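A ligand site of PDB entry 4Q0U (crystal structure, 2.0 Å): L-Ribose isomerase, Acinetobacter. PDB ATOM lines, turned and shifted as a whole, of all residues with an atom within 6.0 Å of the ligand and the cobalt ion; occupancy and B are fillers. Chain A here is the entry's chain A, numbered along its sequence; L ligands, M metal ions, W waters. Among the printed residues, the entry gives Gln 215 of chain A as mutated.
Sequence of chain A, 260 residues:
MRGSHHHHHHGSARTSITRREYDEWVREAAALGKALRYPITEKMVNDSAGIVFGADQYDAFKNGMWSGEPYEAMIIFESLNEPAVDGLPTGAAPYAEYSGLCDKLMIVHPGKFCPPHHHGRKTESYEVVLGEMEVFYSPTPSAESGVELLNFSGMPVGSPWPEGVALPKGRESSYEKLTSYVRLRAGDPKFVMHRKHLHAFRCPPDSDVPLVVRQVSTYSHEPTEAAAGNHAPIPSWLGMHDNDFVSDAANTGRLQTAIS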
ATOM      1  N   ILE A  51      -0.843  -9.888  11.519  1.00  0.00           N
ATOM      2  CA  ILE A  51      -2.134 -10.475  11.911  1.00  0.00           C
ATOM      3  C   ILE A  51      -2.049 -11.403  13.118  1.00  0.00           C
ATOM      4  O   ILE A  51      -1.162 -12.245  13.224  1.00  0.00           O
ATOM      5  CB  ILE A  51      -2.736 -11.257  10.721  1.00  0.00           C
ATOM      6  CG1 ILE A  51      -2.802 -10.344   9.491  1.00  0.00           C
ATOM      7  CG2 ILE A  51      -4.126 -11.764  11.069  1.00  0.00           C
ATOM      8  CD1 ILE A  51      -2.955 -11.077   8.173  1.00  0.00           C
ATOM      9  N   PHE A  53      -4.681 -13.944  15.019  1.00  0.00           N
ATOM     10  CA  PHE A  53      -5.997 -14.565  14.877  1.00  0.00           C
ATOM     11  C   PHE A  53      -6.768 -14.883  16.156  1.00  0.00           C
ATOM     12  O   PHE A  53      -6.900 -16.037  16.539  1.00  0.00           O
ATOM     13  CB  PHE A  53      -5.886 -15.844  14.027  1.00  0.00           C
ATOM     14  CG  PHE A  53      -5.290 -15.622  12.668  1.00  0.00           C
ATOM     15  CD1 PHE A  53      -3.915 -15.738  12.469  1.00  0.00           C
ATOM     16  CD2 PHE A  53      -6.100 -15.309  11.578  1.00  0.00           C
ATOM     17  CE1 PHE A  53      -3.356 -15.535  11.199  1.00  0.00           C
ATOM     18  CE2 PHE A  53      -5.551 -15.107  10.305  1.00  0.00           C
ATOM     19  CZ  PHE A  53      -4.179 -15.220  10.115  1.00  0.00           C
ATOM     20  N   MET A  74       0.579 -14.152  12.010  1.00  0.00           N
ATOM     21  CA  MET A  74       1.456 -14.082  10.841  1.00  0.00           C
ATOM     22  C   MET A  74       1.472 -12.702  10.221  1.00  0.00           C
ATOM     23  O   MET A  74       0.676 -11.823  10.573  1.00  0.00           O
ATOM     24  CB  MET A  74       0.970 -15.074   9.787  1.00  0.00           C
ATOM     25  CG  MET A  74      -0.289 -14.588   9.085  1.00  0.00           C
ATOM     26  SD  MET A  74      -1.077 -15.836   8.066  1.00  0.00           S
ATOM     27  CE  MET A  74       0.112 -15.990   6.724  1.00  0.00           C
ATOM     28  N   ILE A  76       1.502 -10.511   6.519  1.00  0.00           N
ATOM     29  CA  ILE A  76       1.219 -10.600   5.105  1.00  0.00           C
ATOM     30  C   ILE A  76       1.412  -9.241   4.431  1.00  0.00           C
ATOM     31  O   ILE A  76       0.826  -8.237   4.847  1.00  0.00           O
ATOM     32  CB  ILE A  76      -0.226 -11.092   4.832  1.00  0.00           C
ATOM     33  CG1 ILE A  76      -0.396 -12.512   5.387  1.00  0.00           C
ATOM     34  CG2 ILE A  76      -0.518 -11.057   3.339  1.00  0.00           C
ATOM     35  CD1 ILE A  76      -1.785 -13.095   5.199  1.00  0.00           C
ATOM     36  N   LYS A 104       1.069 -12.010  -2.605  1.00  0.00           N
ATOM     37  CA  LYS A 104       1.391 -11.651  -1.232  1.00  0.00           C
ATOM     38  C   LYS A 104       2.621 -12.390  -0.750  1.00  0.00           C
ATOM     39  O   LYS A 104       2.921 -13.488  -1.231  1.00  0.00           O
ATOM     40  CB  LYS A 104       0.248 -12.041  -0.283  1.00  0.00           C
ATOM     41  CG  LYS A 104      -1.114 -11.478  -0.594  1.00  0.00           C
ATOM     42  CD  LYS A 104      -2.143 -12.063   0.390  1.00  0.00           C
ATOM     43  CE  LYS A 104      -3.540 -11.511   0.156  1.00  0.00           C
ATOM     44  NZ  LYS A 104      -4.519 -12.153   1.073  1.00  0.00           N
ATOM     45  N   MET A 106       4.157 -13.986   2.653  1.00  0.00           N
ATOM     46  CA  MET A 106       3.722 -14.365   3.989  1.00  0.00           C
ATOM     47  C   MET A 106       4.931 -14.722   4.837  1.00  0.00           C
ATOM     48  O   MET A 106       5.835 -15.436   4.394  1.00  0.00           O
ATOM     49  CB  MET A 106       2.753 -15.565   3.938  1.00  0.00           C
ATOM     50  CG  MET A 106       1.643 -15.424   2.885  1.00  0.00           C
ATOM     51  SD  MET A 106       0.412 -16.767   2.942  1.00  0.00           S
ATOM     52  CE  MET A 106       1.415 -18.157   2.473  1.00  0.00           C
ATOM     53  N   CYS A 114      -0.789 -20.283  10.394  1.00  0.00           N
ATOM     54  CA  CYS A 114      -1.785 -19.545   9.645  1.00  0.00           C
ATOM     55  C   CYS A 114      -2.864 -20.595   9.986  1.00  0.00           C
ATOM     56  O   CYS A 114      -2.719 -21.770   9.622  1.00  0.00           O
ATOM     57  CB  CYS A 114      -1.528 -19.564   8.140  1.00  0.00           C
ATOM     58  SG  CYS A 114      -2.922 -18.875   7.232  1.00  0.00           S
ATOM     59  N   PRO A 115      -3.928 -20.196  10.702  1.00  0.00           N
ATOM     60  CA  PRO A 115      -4.997 -21.127  11.104  1.00  0.00           C
ATOM     61  C   PRO A 115      -5.907 -21.790  10.081  1.00  0.00           C
ATOM     62  O   PRO A 115      -6.107 -21.293   8.974  1.00  0.00           O
ATOM     63  CB  PRO A 115      -5.782 -20.294  12.124  1.00  0.00           C
ATOM     64  CG  PRO A 115      -5.703 -18.934  11.542  1.00  0.00           C
ATOM     65  CD  PRO A 115      -4.247 -18.816  11.117  1.00  0.00           C
ATOM     66  N   HIS A 117      -8.672 -22.879   7.745  1.00  0.00           N
ATOM     67  CA  HIS A 117      -9.719 -22.110   7.079  1.00  0.00           C
ATOM     68  C   HIS A 117      -9.830 -22.564   5.641  1.00  0.00           C
ATOM     69  O   HIS A 117      -8.998 -23.335   5.144  1.00  0.00           O
ATOM     70  CB  HIS A 117      -9.399 -20.609   7.111  1.00  0.00           C
ATOM     71  CG  HIS A 117      -8.221 -20.227   6.252  1.00  0.00           C
ATOM     72  ND1 HIS A 117      -6.916 -20.426   6.659  1.00  0.00           N
ATOM     73  CD2 HIS A 117      -8.159 -19.697   5.010  1.00  0.00           C
ATOM     74  CE1 HIS A 117      -6.105 -20.037   5.692  1.00  0.00           C
ATOM     75  NE2 HIS A 117      -6.830 -19.587   4.685  1.00  0.00           N
ATOM     76  N   HIS A 118     -10.884 -22.108   4.964  1.00  0.00           N
ATOM     77  CA  HIS A 118     -11.074 -22.420   3.561  1.00  0.00           C
ATOM     78  C   HIS A 118     -11.718 -21.215   2.916  1.00  0.00           C
ATOM     79  O   HIS A 118     -12.264 -20.347   3.609  1.00  0.00           O
ATOM     80  CB  HIS A 118     -11.927 -23.684   3.371  1.00  0.00           C
ATOM     81  CG  HIS A 118     -13.408 -23.476   3.575  1.00  0.00           C
ATOM     82  ND1 HIS A 118     -13.999 -23.480   4.817  1.00  0.00           N
ATOM     83  CD2 HIS A 118     -14.396 -23.272   2.679  1.00  0.00           C
ATOM     84  CE1 HIS A 118     -15.303 -23.295   4.675  1.00  0.00           C
ATOM     85  NE2 HIS A 118     -15.578 -23.165   3.393  1.00  0.00           N
ATOM     86  N   HIS A 119     -11.629 -21.127   1.598  1.00  0.00           N
ATOM     87  CA  HIS A 119     -12.212 -20.017   0.858  1.00  0.00           C
ATOM     88  C   HIS A 119     -13.209 -20.598  -0.118  1.00  0.00           C
ATOM     89  O   HIS A 119     -12.954 -21.639  -0.738  1.00  0.00           O
ATOM     90  CB  HIS A 119     -11.123 -19.289   0.066  1.00  0.00           C
ATOM     91  CG  HIS A 119      -9.958 -18.856   0.898  1.00  0.00           C
ATOM     92  ND1 HIS A 119     -10.003 -17.756   1.729  1.00  0.00           N
ATOM     93  CD2 HIS A 119      -8.729 -19.398   1.059  1.00  0.00           C
ATOM     94  CE1 HIS A 119      -8.847 -17.642   2.365  1.00  0.00           C
ATOM     95  NE2 HIS A 119      -8.062 -18.622   1.980  1.00  0.00           N
ATOM     96  N   LYS A 122     -11.578 -18.278  -3.489  1.00  0.00           N
ATOM     97  CA  LYS A 122     -10.144 -18.169  -3.744  1.00  0.00           C
ATOM     98  C   LYS A 122      -9.311 -19.454  -3.787  1.00  0.00           C
ATOM     99  O   LYS A 122      -9.354 -20.273  -2.869  1.00  0.00           O
ATOM    100  CB  LYS A 122      -9.525 -17.206  -2.734  1.00  0.00           C
ATOM    101  CG  LYS A 122      -8.052 -16.868  -3.022  1.00  0.00           C
ATOM    102  CD  LYS A 122      -7.483 -15.909  -1.985  1.00  0.00           C
ATOM    103  CE  LYS A 122      -7.246 -16.618  -0.660  1.00  0.00           C
ATOM    104  NZ  LYS A 122      -6.619 -15.727   0.349  1.00  0.00           N
ATOM    105  N   GLU A 124      -5.409 -20.806  -4.058  1.00  0.00           N
ATOM    106  CA  GLU A 124      -4.058 -20.347  -3.744  1.00  0.00           C
ATOM    107  C   GLU A 124      -2.955 -21.248  -4.288  1.00  0.00           C
ATOM    108  O   GLU A 124      -3.214 -22.370  -4.697  1.00  0.00           O
ATOM    109  CB  GLU A 124      -3.847 -20.313  -2.221  1.00  0.00           C
ATOM    110  CG  GLU A 124      -4.655 -19.316  -1.445  1.00  0.00           C
ATOM    111  CD  GLU A 124      -4.682 -19.636   0.050  1.00  0.00           C
ATOM    112  OE1 GLU A 124      -3.714 -20.251   0.552  1.00  0.00           O
ATOM    113  OE2 GLU A 124      -5.673 -19.279   0.714  1.00  0.00           O
ATOM    114  N   TYR A 126       1.496 -21.911  -3.407  1.00  0.00           N
ATOM    115  CA  TYR A 126       2.599 -21.549  -2.525  1.00  0.00           C
ATOM    116  C   TYR A 126       3.980 -21.779  -3.128  1.00  0.00           C
ATOM    117  O   TYR A 126       4.234 -22.789  -3.789  1.00  0.00           O
ATOM    118  CB  TYR A 126       2.534 -22.351  -1.217  1.00  0.00           C
ATOM    119  CG  TYR A 126       1.160 -22.448  -0.595  1.00  0.00           C
ATOM    120  CD1 TYR A 126       0.422 -21.296  -0.312  1.00  0.00           C
ATOM    121  CD2 TYR A 126       0.604 -23.688  -0.274  1.00  0.00           C
ATOM    122  CE1 TYR A 126      -0.851 -21.383   0.255  1.00  0.00           C
ATOM    123  CE2 TYR A 126      -0.659 -23.784   0.300  1.00  0.00           C
ATOM    124  CZ  TYR A 126      -1.382 -22.626   0.564  1.00  0.00           C
ATOM    125  OH  TYR A 126      -2.632 -22.724   1.131  1.00  0.00           O
ATOM    126  N   HIS A 199      -7.361 -25.626   4.893  1.00  0.00           N
ATOM    127  CA  HIS A 199      -5.909 -25.606   4.938  1.00  0.00           C
ATOM    128  C   HIS A 199      -5.364 -24.724   6.040  1.00  0.00           C
ATOM    129  O   HIS A 199      -6.037 -23.808   6.523  1.00  0.00           O
ATOM    130  CB  HIS A 199      -5.318 -25.155   3.585  1.00  0.00           C
ATOM    131  CG  HIS A 199      -5.748 -23.791   3.139  1.00  0.00           C
ATOM    132  ND1 HIS A 199      -6.996 -23.540   2.608  1.00  0.00           N
ATOM    133  CD2 HIS A 199      -5.098 -22.602   3.135  1.00  0.00           C
ATOM    134  CE1 HIS A 199      -7.092 -22.258   2.299  1.00  0.00           C
ATOM    135  NE2 HIS A 199      -5.956 -21.669   2.614  1.00  0.00           N
ATOM    136  N   PHE A 201      -1.054 -23.900   7.861  1.00  0.00           N
ATOM    137  CA  PHE A 201       0.363 -24.176   7.717  1.00  0.00           C
ATOM    138  C   PHE A 201       1.159 -23.513   8.831  1.00  0.00           C
ATOM    139  O   PHE A 201       0.679 -22.598   9.502  1.00  0.00           O
ATOM    140  CB  PHE A 201       0.859 -23.726   6.331  1.00  0.00           C
ATOM    141  CG  PHE A 201       0.573 -22.278   6.002  1.00  0.00           C
ATOM    142  CD1 PHE A 201       1.451 -21.271   6.395  1.00  0.00           C
ATOM    143  CD2 PHE A 201      -0.538 -21.937   5.246  1.00  0.00           C
ATOM    144  CE1 PHE A 201       1.205 -19.932   6.041  1.00  0.00           C
ATOM    145  CE2 PHE A 201      -0.790 -20.610   4.882  1.00  0.00           C
ATOM    146  CZ  PHE A 201       0.088 -19.603   5.275  1.00  0.00           C
ATOM    147  N   GLN A 215       2.744 -16.113  -2.032  1.00  0.00           N
ATOM    148  CA  GLN A 215       1.440 -16.668  -2.360  1.00  0.00           C
ATOM    149  C   GLN A 215       0.872 -15.995  -3.596  1.00  0.00           C
ATOM    150  O   GLN A 215       0.787 -14.764  -3.660  1.00  0.00           O
ATOM    151  CB  GLN A 215       0.446 -16.496  -1.205  1.00  0.00           C
ATOM    152  CG  GLN A 215      -0.892 -17.221  -1.470  1.00  0.00           C
ATOM    153  CD  GLN A 215      -2.034 -16.744  -0.605  1.00  0.00           C
ATOM    154  OE1 GLN A 215      -1.901 -16.617   0.607  1.00  0.00           O
ATOM    155  NE2 GLN A 215      -3.178 -16.494  -1.230  1.00  0.00           N
ATOM    156  N   SER A 217      -2.517 -16.107  -5.817  1.00  0.00           N
ATOM    157  CA  SER A 217      -3.866 -16.642  -5.785  1.00  0.00           C
ATOM    158  C   SER A 217      -4.820 -15.770  -6.574  1.00  0.00           C
ATOM    159  O   SER A 217      -4.418 -14.748  -7.134  1.00  0.00           O
ATOM    160  CB  SER A 217      -4.358 -16.696  -4.344  1.00  0.00           C
ATOM    161  OG  SER A 217      -4.672 -15.388  -3.887  1.00  0.00           O
ATOM    162  N   SER A 220      -8.425 -11.639  -3.540  1.00  0.00           N
ATOM    163  CA  SER A 220      -8.617 -11.803  -2.108  1.00  0.00           C
ATOM    164  C   SER A 220      -9.708 -10.864  -1.581  1.00  0.00           C
ATOM    165  O   SER A 220      -9.473  -9.675  -1.349  1.00  0.00           O
ATOM    166  CB  SER A 220      -7.290 -11.551  -1.393  1.00  0.00           C
ATOM    167  OG  SER A 220      -7.342 -11.927  -0.033  1.00  0.00           O
ATOM    168  N   GLU A 222     -11.497  -9.372   1.123  1.00  0.00           N
ATOM    169  CA  GLU A 222     -11.326  -9.216   2.569  1.00  0.00           C
ATOM    170  C   GLU A 222     -11.611  -7.814   3.067  1.00  0.00           C
ATOM    171  O   GLU A 222     -10.740  -6.937   3.033  1.00  0.00           O
ATOM    172  CB  GLU A 222      -9.885  -9.599   2.972  1.00  0.00           C
ATOM    173  CG  GLU A 222      -9.461 -11.003   2.533  1.00  0.00           C
ATOM    174  CD  GLU A 222      -8.052 -11.353   2.992  1.00  0.00           C
ATOM    175  OE1 GLU A 222      -7.106 -10.601   2.667  1.00  0.00           O
ATOM    176  OE2 GLU A 222      -7.892 -12.392   3.677  1.00  0.00           O
ATOM    177  N   ASN A 243     -13.372 -15.672   3.647  1.00  0.00           N
ATOM    178  CA  ASN A 243     -12.488 -16.379   4.567  1.00  0.00           C
ATOM    179  C   ASN A 243     -13.299 -17.065   5.662  1.00  0.00           C
ATOM    180  O   ASN A 243     -13.935 -16.406   6.473  1.00  0.00           O
ATOM    181  CB  ASN A 243     -11.486 -15.409   5.208  1.00  0.00           C
ATOM    182  CG  ASN A 243     -10.705 -14.615   4.173  1.00  0.00           C
ATOM    183  OD1 ASN A 243     -10.223 -15.168   3.184  1.00  0.00           O
ATOM    184  ND2 ASN A 243     -10.555 -13.314   4.402  1.00  0.00           N
ATOM    185  N   PHE A 245     -12.886 -19.403   8.793  1.00  0.00           N
ATOM    186  CA  PHE A 245     -12.016 -20.054   9.770  1.00  0.00           C
ATOM    187  C   PHE A 245     -12.746 -21.140  10.547  1.00  0.00           C
ATOM    188  O   PHE A 245     -13.885 -20.951  10.973  1.00  0.00           O
ATOM    189  CB  PHE A 245     -11.455 -19.000  10.737  1.00  0.00           C
ATOM    190  CG  PHE A 245     -10.417 -18.106  10.115  1.00  0.00           C
ATOM    191  CD1 PHE A 245      -9.099 -18.540   9.965  1.00  0.00           C
ATOM    192  CD2 PHE A 245     -10.765 -16.857   9.617  1.00  0.00           C
ATOM    193  CE1 PHE A 245      -8.154 -17.743   9.334  1.00  0.00           C
ATOM    194  CE2 PHE A 245      -9.830 -16.050   8.981  1.00  0.00           C
ATOM    195  CZ  PHE A 245      -8.524 -16.493   8.840  1.00  0.00           C
ATOM    196  N   ARG A 254      -9.061 -11.227  12.999  1.00  0.00           N
ATOM    197  CA  ARG A 254      -8.394 -11.399  11.708  1.00  0.00           C
ATOM    198  C   ARG A 254      -8.440 -10.097  10.911  1.00  0.00           C
ATOM    199  O   ARG A 254      -7.532  -9.803  10.132  1.00  0.00           O
ATOM    200  CB  ARG A 254      -9.067 -12.524  10.916  1.00  0.00           C
ATOM    201  CG  ARG A 254      -8.252 -13.094   9.753  1.00  0.00           C
ATOM    202  CD  ARG A 254      -8.042 -12.100   8.622  1.00  0.00           C
ATOM    203  NE  ARG A 254      -7.209 -12.654   7.560  1.00  0.00           N
ATOM    204  CZ  ARG A 254      -6.727 -11.957   6.532  1.00  0.00           C
ATOM    205  NH1 ARG A 254      -5.987 -12.550   5.610  1.00  0.00           N
ATOM    206  NH2 ARG A 254      -6.997 -10.657   6.430  1.00  0.00           N
HETATM  207  C1  LIG L   1      -4.625 -16.024   5.481  1.00  0.00           C
HETATM  208  O1  LIG L   1      -5.426 -15.506   6.520  1.00  0.00           O
HETATM  209  C2  LIG L   1      -4.692 -15.094   4.280  1.00  0.00           C
HETATM  210  O2  LIG L   1      -6.051 -14.877   3.904  1.00  0.00           O
HETATM  211  C3  LIG L   1      -3.899 -15.681   3.093  1.00  0.00           C
HETATM  212  O3  LIG L   1      -3.969 -14.774   2.005  1.00  0.00           O
HETATM  213  C4  LIG L   1      -4.396 -17.063   2.654  1.00  0.00           C
HETATM  214  O4  LIG L   1      -5.798 -17.156   2.808  1.00  0.00           O
HETATM  215  C5  LIG L   1      -3.709 -18.164   3.461  1.00  0.00           C
HETATM  216  O5  LIG L   1      -3.925 -19.359   3.205  1.00  0.00           O
HETATM  217 CO    CO M   1      -6.152 -19.330   2.572  1.00  0.00          CO
HETATM  218  O   HOH W   1      -4.633 -14.480  -0.868  1.00  0.00           O
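The side-chain amino group of Lys 104 lies within hydrogen-bond range of an oxygen (O3) of the ligand (2.8 Å). The guanidinium group of Arg 254 lies within hydrogen-bond range of an oxygen (O2) of the ligand (2.9 Å). O3 of the ligand lies within hydrogen-bond range of NZ of Lys 122. OE2 of Glu 222 lies within hydrogen-bond range of O2 of the ligand (3.1 Å). O3 of the ligand sits at hydrogen-bond distance from OE1 of Gln 215, at 3.1 Å.
The side-chain carboxylate (OE1) of Glu 124 lies within hydrogen-bond range of the side-chain hydroxyl (OH) of Tyr 126, 2.8 Å away. The side-chain amide oxygen of Asn 243 sits close to a ring nitrogen (ND1) of His 119 (3.0 Å). O of Pro 115 is in hydrogen-bond range of ND1 of His 117 (2.6 Å). The side-chain amino group (NZ) of Lys 104 is in salt-bridge range of the side-chain carboxylate (OE1) of Glu 222. The side-chain carboxylate of Glu 222 lies within hydrogen-bond range of the side-chain hydroxyl of Ser 220 (3.0 Å). The side-chain sulfur (SD) of Met 106 sits close to the side-chain amide oxygen (OE1) of Gln 215 (3.3 Å). OG of Ser 217 lies within hydrogen-bond range of NE2 of Gln 215 (3.2 Å). The backbone NH (N) of Cys 114 sits at hydrogen-bond distance from the backbone carbonyl oxygen (O) of Phe 201, at 2.9 Å.
Residues that only touch the ligand: Ile 76 (3.6 Å), Cys 114 (3.8 Å), Phe 201 (3.8 Å), Phe 53 (3.8 Å) and Phe 245 (3.99 Å). Hydrophobic or aromatic side chains within 4 Å of the ligand: Phe 53, Ile 76, His 117, His 119, His 199, Phe 201 and Phe 245. Along chain A the residues within 4 Å of the ligand span positions 53 to 254.
OE2 of Glu 124 binds the cobalt ion. The cobalt ion is bound by NE2 of His 119 (2.1 Å). O4 of the ligand binds the cobalt ion (2.2 Å). NE2 of His 117 binds the cobalt ion (2.2 Å). An oxygen (O5) of the ligand binds the cobalt ion. The cobalt ion is bound by NE2 of His 199, at 2.3 Å. The cobalt ion has six donor atoms within binding distance.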
